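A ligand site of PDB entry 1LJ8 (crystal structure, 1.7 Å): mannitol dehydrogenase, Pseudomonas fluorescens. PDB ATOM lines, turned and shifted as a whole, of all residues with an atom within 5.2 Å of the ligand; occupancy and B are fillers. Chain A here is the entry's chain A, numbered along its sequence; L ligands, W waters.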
ATOM      1  N   ILE A  32      36.015   3.850   0.727  1.00  0.00           N
ATOM      2  CA  ILE A  32      35.302   2.581   0.849  1.00  0.00           C
ATOM      3  C   ILE A  32      34.202   2.475  -0.207  1.00  0.00           C
ATOM      4  O   ILE A  32      33.258   3.302  -0.248  1.00  0.00           O
ATOM      5  CB  ILE A  32      34.699   2.418   2.249  1.00  0.00           C
ATOM      6  CG1 ILE A  32      35.817   2.581   3.299  1.00  0.00           C
ATOM      7  CG2 ILE A  32      34.025   0.995   2.361  1.00  0.00           C
ATOM      8  CD1 ILE A  32      35.291   2.466   4.771  1.00  0.00           C
ATOM      9  N   GLY A  33      34.307   1.436  -1.033  1.00  0.00           N
ATOM     10  CA  GLY A  33      33.320   1.211  -2.092  1.00  0.00           C
ATOM     11  C   GLY A  33      33.846   1.719  -3.438  1.00  0.00           C
ATOM     12  O   GLY A  33      33.289   2.658  -4.013  1.00  0.00           O
ATOM     13  N   VAL A  34      34.874   1.099  -3.985  1.00  0.00           N
ATOM     14  CA  VAL A  34      35.404   1.607  -5.253  1.00  0.00           C
ATOM     15  C   VAL A  34      34.588   1.039  -6.411  1.00  0.00           C
ATOM     16  O   VAL A  34      34.845  -0.086  -6.854  1.00  0.00           O
ATOM     17  CB  VAL A  34      36.898   1.215  -5.432  1.00  0.00           C
ATOM     18  CG1 VAL A  34      37.443   1.775  -6.814  1.00  0.00           C
ATOM     19  CG2 VAL A  34      37.717   1.805  -4.257  1.00  0.00           C
ATOM     20  N   GLY A  35      33.617   1.813  -6.893  1.00  0.00           N
ATOM     21  CA  GLY A  35      32.801   1.376  -8.009  1.00  0.00           C
ATOM     22  C   GLY A  35      32.995   2.366  -9.143  1.00  0.00           C
ATOM     23  O   GLY A  35      34.123   2.879  -9.358  1.00  0.00           O
ATOM     24  N   GLY A  36      31.906   2.618  -9.872  1.00  0.00           N
ATOM     25  CA  GLY A  36      32.011   3.571 -10.952  1.00  0.00           C
ATOM     26  C   GLY A  36      31.965   5.020 -10.481  1.00  0.00           C
ATOM     27  O   GLY A  36      32.815   5.835 -10.842  1.00  0.00           O
ATOM     28  N   PHE A  37      30.992   5.353  -9.644  1.00  0.00           N
ATOM     29  CA  PHE A  37      30.854   6.761  -9.251  1.00  0.00           C
ATOM     30  C   PHE A  37      32.052   7.362  -8.561  1.00  0.00           C
ATOM     31  O   PHE A  37      32.468   8.478  -8.849  1.00  0.00           O
ATOM     32  CB  PHE A  37      29.606   6.955  -8.362  1.00  0.00           C
ATOM     33  CG  PHE A  37      29.328   8.397  -8.072  1.00  0.00           C
ATOM     34  CD1 PHE A  37      29.056   9.301  -9.111  1.00  0.00           C
ATOM     35  CD2 PHE A  37      29.404   8.868  -6.780  1.00  0.00           C
ATOM     36  CE1 PHE A  37      28.867  10.685  -8.824  1.00  0.00           C
ATOM     37  CE2 PHE A  37      29.210  10.216  -6.457  1.00  0.00           C
ATOM     38  CZ  PHE A  37      28.948  11.135  -7.484  1.00  0.00           C
ATOM     39  N   HIS A  38      32.654   6.614  -7.642  1.00  0.00           N
ATOM     40  CA  HIS A  38      33.838   7.154  -6.975  1.00  0.00           C
ATOM     41  C   HIS A  38      34.893   7.539  -7.998  1.00  0.00           C
ATOM     42  O   HIS A  38      35.526   8.594  -7.914  1.00  0.00           O
ATOM     43  CB  HIS A  38      34.473   6.101  -6.035  1.00  0.00           C
ATOM     44  CG  HIS A  38      35.846   6.488  -5.584  1.00  0.00           C
ATOM     45  ND1 HIS A  38      36.056   7.535  -4.712  1.00  0.00           N
ATOM     46  CD2 HIS A  38      37.069   6.027  -5.939  1.00  0.00           C
ATOM     47  CE1 HIS A  38      37.361   7.712  -4.556  1.00  0.00           C
ATOM     48  NE2 HIS A  38      37.995   6.814  -5.297  1.00  0.00           N
ATOM     49  N   LEU A  65      35.042  -4.050   0.920  1.00  0.00           N
ATOM     50  CA  LEU A  65      34.563  -4.902   2.047  1.00  0.00           C
ATOM     51  C   LEU A  65      33.775  -6.133   1.588  1.00  0.00           C
ATOM     52  O   LEU A  65      33.415  -6.995   2.427  1.00  0.00           O
ATOM     53  CB  LEU A  65      33.618  -4.083   2.955  1.00  0.00           C
ATOM     54  CG  LEU A  65      34.180  -2.764   3.491  1.00  0.00           C
ATOM     55  CD1 LEU A  65      33.220  -2.150   4.556  1.00  0.00           C
ATOM     56  CD2 LEU A  65      35.582  -3.075   4.134  1.00  0.00           C
ATOM     57  N   ARG A  66      33.510  -6.224   0.296  1.00  0.00           N
ATOM     58  CA  ARG A  66      32.663  -7.307  -0.245  1.00  0.00           C
ATOM     59  C   ARG A  66      33.365  -8.214  -1.218  1.00  0.00           C
ATOM     60  O   ARG A  66      34.320  -7.802  -1.875  1.00  0.00           O
ATOM     61  CB  ARG A  66      31.426  -6.693  -0.926  1.00  0.00           C
ATOM     62  CG  ARG A  66      30.593  -5.846   0.060  1.00  0.00           C
ATOM     63  CD  ARG A  66      29.438  -5.112  -0.607  1.00  0.00           C
ATOM     64  NE  ARG A  66      28.321  -5.933  -1.107  1.00  0.00           N
ATOM     65  CZ  ARG A  66      28.061  -6.182  -2.386  1.00  0.00           C
ATOM     66  NH1 ARG A  66      28.826  -5.695  -3.381  1.00  0.00           N
ATOM     67  NH2 ARG A  66      26.978  -6.889  -2.693  1.00  0.00           N
ATOM     68  N   GLU A  68      32.465  -9.206  -4.068  1.00  0.00           N
ATOM     69  CA  GLU A  68      32.472  -8.693  -5.446  1.00  0.00           C
ATOM     70  C   GLU A  68      33.549  -7.626  -5.736  1.00  0.00           C
ATOM     71  O   GLU A  68      33.821  -7.325  -6.894  1.00  0.00           O
ATOM     72  CB  GLU A  68      31.085  -8.151  -5.877  1.00  0.00           C
ATOM     73  CG  GLU A  68      30.140  -7.732  -4.765  1.00  0.00           C
ATOM     74  CD  GLU A  68      29.524  -8.906  -4.017  1.00  0.00           C
ATOM     75  OE1 GLU A  68      28.670  -9.639  -4.583  1.00  0.00           O
ATOM     76  OE2 GLU A  68      29.905  -9.101  -2.838  1.00  0.00           O
ATOM     77  N   ASP A  69      34.176  -7.078  -4.696  1.00  0.00           N
ATOM     78  CA  ASP A  69      35.225  -6.090  -4.893  1.00  0.00           C
ATOM     79  C   ASP A  69      36.559  -6.691  -5.358  1.00  0.00           C
ATOM     80  O   ASP A  69      37.442  -5.973  -5.800  1.00  0.00           O
ATOM     81  CB  ASP A  69      35.467  -5.313  -3.585  1.00  0.00           C
ATOM     82  CG  ASP A  69      34.227  -4.550  -3.138  1.00  0.00           C
ATOM     83  OD1 ASP A  69      33.466  -4.087  -4.031  1.00  0.00           O
ATOM     84  OD2 ASP A  69      33.984  -4.416  -1.926  1.00  0.00           O
ATOM     85  N   THR A 130      31.312   5.432  -0.855  1.00  0.00           N
ATOM     86  CA  THR A 130      30.186   5.253  -1.802  1.00  0.00           C
ATOM     87  C   THR A 130      29.795   3.784  -1.466  1.00  0.00           C
ATOM     88  O   THR A 130      30.184   2.831  -2.142  1.00  0.00           O
ATOM     89  CB  THR A 130      30.481   5.415  -3.306  1.00  0.00           C
ATOM     90  OG1 THR A 130      31.600   4.640  -3.689  1.00  0.00           O
ATOM     91  CG2 THR A 130      30.760   6.915  -3.633  1.00  0.00           C
ATOM     92  N   ILE A 131      29.061   3.637  -0.366  1.00  0.00           N
ATOM     93  CA  ILE A 131      28.642   2.289   0.122  1.00  0.00           C
ATOM     94  C   ILE A 131      27.183   1.971  -0.201  1.00  0.00           C
ATOM     95  O   ILE A 131      26.624   0.981   0.291  1.00  0.00           O
ATOM     96  CB  ILE A 131      28.833   2.169   1.661  1.00  0.00           C
ATOM     97  CG1 ILE A 131      28.006   3.249   2.410  1.00  0.00           C
ATOM     98  CG2 ILE A 131      30.321   2.350   2.000  1.00  0.00           C
ATOM     99  CD1 ILE A 131      28.017   3.054   3.980  1.00  0.00           C
ATOM    100  N   THR A 132      26.613   2.801  -1.082  1.00  0.00           N
ATOM    101  CA  THR A 132      25.220   2.725  -1.563  1.00  0.00           C
ATOM    102  C   THR A 132      24.170   3.253  -0.599  1.00  0.00           C
ATOM    103  O   THR A 132      24.406   3.386   0.613  1.00  0.00           O
ATOM    104  CB  THR A 132      24.766   1.293  -2.095  1.00  0.00           C
ATOM    105  OG1 THR A 132      24.419   0.427  -0.991  1.00  0.00           O
ATOM    106  CG2 THR A 132      25.853   0.696  -3.015  1.00  0.00           C
ATOM    107  N   GLU A 133      22.990   3.537  -1.165  1.00  0.00           N
ATOM    108  CA  GLU A 133      21.884   4.135  -0.437  1.00  0.00           C
ATOM    109  C   GLU A 133      21.431   3.395   0.818  1.00  0.00           C
ATOM    110  O   GLU A 133      21.021   4.048   1.806  1.00  0.00           O
ATOM    111  CB  GLU A 133      20.663   4.315  -1.368  1.00  0.00           C
ATOM    112  CG  GLU A 133      20.842   5.381  -2.492  1.00  0.00           C
ATOM    113  CD  GLU A 133      21.613   4.959  -3.722  1.00  0.00           C
ATOM    114  OE1 GLU A 133      22.164   3.831  -3.790  1.00  0.00           O
ATOM    115  OE2 GLU A 133      21.676   5.775  -4.677  1.00  0.00           O
ATOM    116  N   GLY A 135      23.483   1.358   2.589  1.00  0.00           N
ATOM    117  CA  GLY A 135      24.612   0.940   3.438  1.00  0.00           C
ATOM    118  C   GLY A 135      24.719   1.560   4.823  1.00  0.00           C
ATOM    119  O   GLY A 135      25.543   1.133   5.636  1.00  0.00           O
ATOM    120  N   VAL A 165      31.386  -1.222   7.365  1.00  0.00           N
ATOM    121  CA  VAL A 165      32.041   0.055   7.394  1.00  0.00           C
ATOM    122  C   VAL A 165      32.115   0.610   8.833  1.00  0.00           C
ATOM    123  O   VAL A 165      33.105   1.237   9.238  1.00  0.00           O
ATOM    124  CB  VAL A 165      31.286   1.022   6.394  1.00  0.00           C
ATOM    125  CG1 VAL A 165      29.824   1.132   6.793  1.00  0.00           C
ATOM    126  CG2 VAL A 165      31.915   2.371   6.407  1.00  0.00           C
ATOM    127  N   CYS A 189      29.689  10.150   0.020  1.00  0.00           N
ATOM    128  CA  CYS A 189      29.426  10.591  -1.357  1.00  0.00           C
ATOM    129  C   CYS A 189      28.260   9.759  -1.901  1.00  0.00           C
ATOM    130  O   CYS A 189      28.159   9.511  -3.113  1.00  0.00           O
ATOM    131  CB  CYS A 189      30.674  10.397  -2.245  1.00  0.00           C
ATOM    132  SG  CYS A 189      32.028  11.440  -1.687  1.00  0.00           S
ATOM    133  N   ASP A 190      27.364   9.334  -1.013  1.00  0.00           N
ATOM    134  CA  ASP A 190      26.177   8.596  -1.441  1.00  0.00           C
ATOM    135  C   ASP A 190      24.938   9.480  -1.580  1.00  0.00           C
ATOM    136  O   ASP A 190      24.873  10.584  -1.026  1.00  0.00           O
ATOM    137  CB  ASP A 190      25.866   7.438  -0.459  1.00  0.00           C
ATOM    138  CG  ASP A 190      26.862   6.275  -0.605  1.00  0.00           C
ATOM    139  OD1 ASP A 190      26.843   5.668  -1.716  1.00  0.00           O
ATOM    140  OD2 ASP A 190      27.622   5.953   0.377  1.00  0.00           O
ATOM    141  N   ASN A 191      23.949   8.970  -2.302  1.00  0.00           N
ATOM    142  CA  ASN A 191      22.713   9.703  -2.551  1.00  0.00           C
ATOM    143  C   ASN A 191      21.726   9.625  -1.401  1.00  0.00           C
ATOM    144  O   ASN A 191      20.764   8.860  -1.468  1.00  0.00           O
ATOM    145  CB  ASN A 191      22.041   9.106  -3.795  1.00  0.00           C
ATOM    146  CG  ASN A 191      22.772   9.444  -5.076  1.00  0.00           C
ATOM    147  OD1 ASN A 191      23.420  10.498  -5.201  1.00  0.00           O
ATOM    148  ND2 ASN A 191      22.586   8.588  -6.079  1.00  0.00           N
ATOM    149  N   VAL A 229      26.460  15.373  -4.607  1.00  0.00           N
ATOM    150  CA  VAL A 229      27.409  14.800  -5.561  1.00  0.00           C
ATOM    151  C   VAL A 229      26.631  14.425  -6.797  1.00  0.00           C
ATOM    152  O   VAL A 229      25.565  13.799  -6.705  1.00  0.00           O
ATOM    153  CB  VAL A 229      28.139  13.573  -4.938  1.00  0.00           C
ATOM    154  CG1 VAL A 229      28.916  14.085  -3.667  1.00  0.00           C
ATOM    155  CG2 VAL A 229      27.133  12.462  -4.572  1.00  0.00           C
ATOM    156  N   ASP A 230      27.127  14.810  -7.983  1.00  0.00           N
ATOM    157  CA  ASP A 230      26.311  14.567  -9.147  1.00  0.00           C
ATOM    158  C   ASP A 230      27.137  14.252 -10.398  1.00  0.00           C
ATOM    159  O   ASP A 230      27.947  15.078 -10.798  1.00  0.00           O
ATOM    160  CB  ASP A 230      25.484  15.856  -9.403  1.00  0.00           C
ATOM    161  CG  ASP A 230      24.318  15.658 -10.375  1.00  0.00           C
ATOM    162  OD1 ASP A 230      24.111  14.527 -10.812  1.00  0.00           O
ATOM    163  OD2 ASP A 230      23.589  16.642 -10.705  1.00  0.00           O
ATOM    164  N   ARG A 231      26.960  13.062 -10.962  1.00  0.00           N
ATOM    165  CA  ARG A 231      27.592  12.700 -12.249  1.00  0.00           C
ATOM    166  C   ARG A 231      27.056  11.330 -12.622  1.00  0.00           C
ATOM    167  O   ARG A 231      27.371  10.334 -11.958  1.00  0.00           O
ATOM    168  CB  ARG A 231      29.132  12.669 -12.215  1.00  0.00           C
ATOM    169  CG  ARG A 231      29.665  12.410 -13.655  1.00  0.00           C
ATOM    170  CD  ARG A 231      31.197  12.485 -13.729  1.00  0.00           C
ATOM    171  NE  ARG A 231      31.532  13.113 -15.013  1.00  0.00           N
ATOM    172  CZ  ARG A 231      32.750  13.472 -15.387  1.00  0.00           C
ATOM    173  NH1 ARG A 231      33.785  13.244 -14.596  1.00  0.00           N
ATOM    174  NH2 ARG A 231      32.908  14.164 -16.528  1.00  0.00           N
ATOM    175  N   ILE A 232      26.226  11.284 -13.664  1.00  0.00           N
ATOM    176  CA  ILE A 232      25.610  10.028 -14.106  1.00  0.00           C
ATOM    177  C   ILE A 232      26.722   9.101 -14.573  1.00  0.00           C
ATOM    178  O   ILE A 232      27.490   9.398 -15.502  1.00  0.00           O
ATOM    179  CB  ILE A 232      24.560  10.279 -15.187  1.00  0.00           C
ATOM    180  CG1 ILE A 232      23.352  11.017 -14.543  1.00  0.00           C
ATOM    181  CG2 ILE A 232      24.076   8.958 -15.782  1.00  0.00           C
ATOM    182  CD1 ILE A 232      22.445  11.728 -15.636  1.00  0.00           C
ATOM    183  N   THR A 233      26.765   7.936 -13.935  1.00  0.00           N
ATOM    184  CA  THR A 233      27.854   6.975 -14.182  1.00  0.00           C
ATOM    185  C   THR A 233      27.274   5.581 -14.390  1.00  0.00           C
ATOM    186  O   THR A 233      26.981   4.846 -13.428  1.00  0.00           O
ATOM    187  CB  THR A 233      28.849   7.015 -12.963  1.00  0.00           C
ATOM    188  OG1 THR A 233      29.339   8.359 -12.763  1.00  0.00           O
ATOM    189  CG2 THR A 233      30.057   6.035 -13.223  1.00  0.00           C
ATOM    190  N   PRO A 234      27.073   5.192 -15.632  1.00  0.00           N
ATOM    191  CA  PRO A 234      26.529   3.864 -15.931  1.00  0.00           C
ATOM    192  C   PRO A 234      27.494   2.732 -15.468  1.00  0.00           C
ATOM    193  O   PRO A 234      28.654   3.007 -15.118  1.00  0.00           O
ATOM    194  CB  PRO A 234      26.457   3.853 -17.470  1.00  0.00           C
ATOM    195  CG  PRO A 234      26.316   5.353 -17.842  1.00  0.00           C
ATOM    196  CD  PRO A 234      27.231   6.039 -16.854  1.00  0.00           C
ATOM    197  N   LYS A 295      18.407  17.736  -5.599  1.00  0.00           N
ATOM    198  CA  LYS A 295      18.875  16.759  -6.571  1.00  0.00           C
ATOM    199  C   LYS A 295      18.273  15.387  -6.321  1.00  0.00           C
ATOM    200  O   LYS A 295      17.858  14.683  -7.247  1.00  0.00           O
ATOM    201  CB  LYS A 295      20.398  16.680  -6.485  1.00  0.00           C
ATOM    202  CG  LYS A 295      20.944  15.635  -7.480  1.00  0.00           C
ATOM    203  CD  LYS A 295      21.718  14.609  -6.787  1.00  0.00           C
ATOM    204  CE  LYS A 295      22.341  13.622  -7.780  1.00  0.00           C
ATOM    205  NZ  LYS A 295      22.274  12.231  -7.201  1.00  0.00           N
ATOM    206  N   ARG A 373      20.631  -0.680 -14.003  1.00  0.00           N
ATOM    207  CA  ARG A 373      21.377   0.015 -12.956  1.00  0.00           C
ATOM    208  C   ARG A 373      20.410   0.902 -12.185  1.00  0.00           C
ATOM    209  O   ARG A 373      20.365   0.876 -10.964  1.00  0.00           O
ATOM    210  CB  ARG A 373      22.471   0.913 -13.565  1.00  0.00           C
ATOM    211  CG  ARG A 373      23.338   1.617 -12.521  1.00  0.00           C
ATOM    212  CD  ARG A 373      24.275   2.662 -13.154  1.00  0.00           C
ATOM    213  NE  ARG A 373      23.512   3.848 -13.524  1.00  0.00           N
ATOM    214  CZ  ARG A 373      23.099   4.756 -12.637  1.00  0.00           C
ATOM    215  NH1 ARG A 373      23.358   4.627 -11.331  1.00  0.00           N
ATOM    216  NH2 ARG A 373      22.426   5.824 -13.073  1.00  0.00           N
HETATM  217  P1  LIG L   1      28.825   0.244  -8.134  1.00  0.00           P
HETATM  218  O1  LIG L   1      27.887  -0.854  -8.177  1.00  0.00           O
HETATM  219  O2  LIG L   1      29.820   0.504  -9.216  1.00  0.00           O
HETATM  220  O3  LIG L   1      29.693   0.172  -6.804  1.00  0.00           O
HETATM  221  C1  LIG L   1      29.030   0.078  -5.511  1.00  0.00           C
HETATM  222  C2  LIG L   1      30.244  -0.113  -4.576  1.00  0.00           C
HETATM  223  O4  LIG L   1      29.718  -0.165  -3.195  1.00  0.00           O
HETATM  224  C3  LIG L   1      30.994  -1.486  -4.691  1.00  0.00           C
HETATM  225  O5  LIG L   1      32.384  -1.211  -4.436  1.00  0.00           O
HETATM  226  C4  LIG L   1      30.323  -2.338  -3.613  1.00  0.00           C
HETATM  227  O6  LIG L   1      31.129  -3.432  -3.185  1.00  0.00           O
HETATM  228  C5  LIG L   1      30.169  -1.317  -2.501  1.00  0.00           C
HETATM  229  N1  LIG L   1      29.196  -1.638  -1.497  1.00  0.00           N
HETATM  230  C6  LIG L   1      27.889  -2.050  -1.599  1.00  0.00           C
HETATM  231  N2  LIG L   1      27.313  -2.195  -0.432  1.00  0.00           N
HETATM  232  C7  LIG L   1      28.308  -1.858   0.472  1.00  0.00           C
HETATM  233  C8  LIG L   1      28.256  -1.819   1.876  1.00  0.00           C
HETATM  234  N3  LIG L   1      27.187  -2.095   2.627  1.00  0.00           N
HETATM  235  N4  LIG L   1      29.409  -1.458   2.555  1.00  0.00           N
HETATM  236  C9  LIG L   1      30.584  -1.142   1.879  1.00  0.00           C
HETATM  237  N5  LIG L   1      30.653  -1.154   0.483  1.00  0.00           N
HETATM  238  C10 LIG L   1      29.468  -1.526  -0.164  1.00  0.00           C
HETATM  239  O7  LIG L   1      27.950   1.538  -7.905  1.00  0.00           O
HETATM  240  P2  LIG L   1      28.213   3.088  -8.268  1.00  0.00           P
HETATM  241  O8  LIG L   1      27.622   3.381  -9.570  1.00  0.00           O
HETATM  242  O9  LIG L   1      29.647   3.329  -8.095  1.00  0.00           O
HETATM  243  O10 LIG L   1      27.328   3.841  -7.199  1.00  0.00           O
HETATM  244  C11 LIG L   1      27.711   3.734  -5.833  1.00  0.00           C
HETATM  245  C12 LIG L   1      26.991   4.797  -5.131  1.00  0.00           C
HETATM  246  O11 LIG L   1      27.460   6.125  -5.445  1.00  0.00           O
HETATM  247  C13 LIG L   1      25.424   4.865  -5.274  1.00  0.00           C
HETATM  248  O12 LIG L   1      24.775   3.866  -4.498  1.00  0.00           O
HETATM  249  C14 LIG L   1      25.110   6.308  -4.930  1.00  0.00           C
HETATM  250  O13 LIG L   1      24.903   6.474  -3.526  1.00  0.00           O
HETATM  251  C15 LIG L   1      26.353   7.078  -5.436  1.00  0.00           C
HETATM  252  N6  LIG L   1      26.197   7.711  -6.755  1.00  0.00           N
HETATM  253  C16 LIG L   1      26.187   7.028  -7.980  1.00  0.00           C
HETATM  254  C17 LIG L   1      25.919   7.758  -9.121  1.00  0.00           C
HETATM  255  C18 LIG L   1      25.873   7.015 -10.469  1.00  0.00           C
HETATM  256  O14 LIG L   1      25.442   7.649 -11.443  1.00  0.00           O
HETATM  257  N7  LIG L   1      26.211   5.748 -10.569  1.00  0.00           N
HETATM  258  C19 LIG L   1      25.646   9.207  -9.058  1.00  0.00           C
HETATM  259  C20 LIG L   1      25.696   9.855  -7.788  1.00  0.00           C
HETATM  260  C21 LIG L   1      25.971   9.122  -6.598  1.00  0.00           C
HETATM  261  O   HOH W   1      24.967   2.506  -9.838  1.00  0.00           O
HETATM  262  O   HOH W   2      28.526   2.810 -12.028  1.00  0.00           O
HETATM  263  O   HOH W   3      33.264  -2.276  -0.376  1.00  0.00           O
HETATM  264  O   HOH W   4      34.972  -1.546  -3.094  1.00  0.00           O
HETATM  265  O   HOH W   5      25.267  -1.013  -6.627  1.00  0.00           O
HETATM  266  O   HOH W   6      33.675  -2.542  -6.768  1.00  0.00           O
HETATM  267  O   HOH W   7      31.530  -1.693  -9.651  1.00  0.00           O
HETATM  268  O   HOH W   8      31.836   4.189  -6.551  1.00  0.00           O
HETATM  269  O   HOH W   9      22.569   5.043  -7.136  1.00  0.00           O
HETATM  270  O   HOH W  10      24.375  -3.433  -0.069  1.00  0.00           O
HETATM  271  O   HOH W  11      29.563  -1.987   5.301  1.00  0.00           O
HETATM  272  O   HOH W  12      24.274  -2.774   2.411  1.00  0.00           O
HETATM  273  O   HOH W  13      26.870  -1.205   5.620  1.00  0.00           O
HETATM  274  O   HOH W  14      25.681  -0.147 -10.216  1.00  0.00           O
HETATM  275  O   HOH W  15      29.955   0.559 -11.969  1.00  0.00           O
HETATM  276  O   HOH W  16      26.577  -2.835  -4.584  1.00  0.00           O
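The side-chain carboxylate (OD2) of Asp 69 sits at hydrogen-bond distance from the backbone NH (N) of Leu 65, 3.1 Å away. The backbone carbonyl oxygen of Gly 33 sits at hydrogen-bond distance from the side-chain hydroxyl of Thr 130 (2.6 Å). OD1 of Asp 190 sits at hydrogen-bond distance from N of Thr 132 (2.9 Å). The side-chain hydroxyl (OG1) of Thr 233 lies within hydrogen-bond range of the backbone carbonyl oxygen (O) of Arg 231 (2.9 Å). The guanidinium group (NH1) of Arg 66 lies within salt-bridge range of the side-chain carboxylate (OE2) of Glu 68 (3.6 Å). The side-chain amide nitrogen (ND2) of Asn 191 lies within hydrogen-bond range of the side-chain carboxylate (OE2) of Glu 133 (3.3 Å). The side-chain amino group (NZ) of Lys 295 is in hydrogen-bond range of the side-chain amide oxygen (OD1) of Asn 191. The side-chain carboxylate (OD2) of Asp 190 is in hydrogen-bond range of the backbone NH (N) of Ile 131.
The side-chain carboxylate of Asp 69 lies within hydrogen-bond range of an oxygen (O6) of the ligand, at 2.6 Å. The side-chain carboxylate (OD1) of Asp 190 lies within hydrogen-bond range of an oxygen (O13) of the ligand (2.8 Å). An oxygen (O9) of the ligand sits at hydrogen-bond distance from the backbone NH (N) of Gly 36 (3.0 Å). The backbone NH (N) of Val 34 is in hydrogen-bond range of an oxygen (O5) of the ligand. The guanidinium group (NH1) of Arg 66 is in hydrogen-bond range of an oxygen (O6) of the ligand. An oxygen (O9) of the ligand lies within hydrogen-bond range of the backbone NH (N) of Phe 37. An oxygen (O13) of the ligand sits at hydrogen-bond distance from the backbone NH of Asn 191, 2.9 Å away. The side-chain carboxylate (OE1) of Glu 133 sits at hydrogen-bond distance from an oxygen (O12) of the ligand (2.7 Å). An oxygen (O14) of the ligand lies within hydrogen-bond range of the backbone NH (N) of Thr 233, at 2.8 Å. A nitrogen (N7) of the ligand is in hydrogen-bond range of the backbone carbonyl oxygen of Thr 233, at 3.1 Å.
O of Thr 130 lies close to O4 of the ligand, 3.2 Å away. O of Ile 131 sits close to N2 of the ligand (3.3 Å). O14 of the ligand lies close to O of Arg 231 (3.3 Å). A nitrogen (N7) of the ligand sits close to the guanidinium group (NH1) of Arg 373, at 3.2 Å. Merely in contact with the ligand: Gly 33, Gly 35, Leu 65, Thr 132, Cys 189 and Ile 232.
Water W11 lies within hydrogen-bond range of a nitrogen (N4) of the ligand (2.8 Å) and the backbone NH of Val 165 (2.9 Å). Water W1 bridges an oxygen (O8) of the ligand and the guanidinium group (NH1) of Arg 373. Water W4 lies within hydrogen-bond range of N of Val 34 (2.8 Å), O5 of the ligand (2.9 Å) and OD1 of Asp 69 (3.1 Å). Water W3 lies within hydrogen-bond range of OD2 of Asp 69 (2.7 Å), N of Leu 65 (2.8 Å) and N5 of the ligand (3.0 Å). Water W6 lies within hydrogen-bond range of the backbone carbonyl oxygen of Val 34 (2.7 Å), an oxygen (O5) of the ligand (3.0 Å) and the side-chain carboxylate of Asp 69 (3.1 Å). Water W13 bridges the backbone carbonyl oxygen (O) of Gly 135 (2.7 Å) and a nitrogen (N3) of the ligand (3.1 Å).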
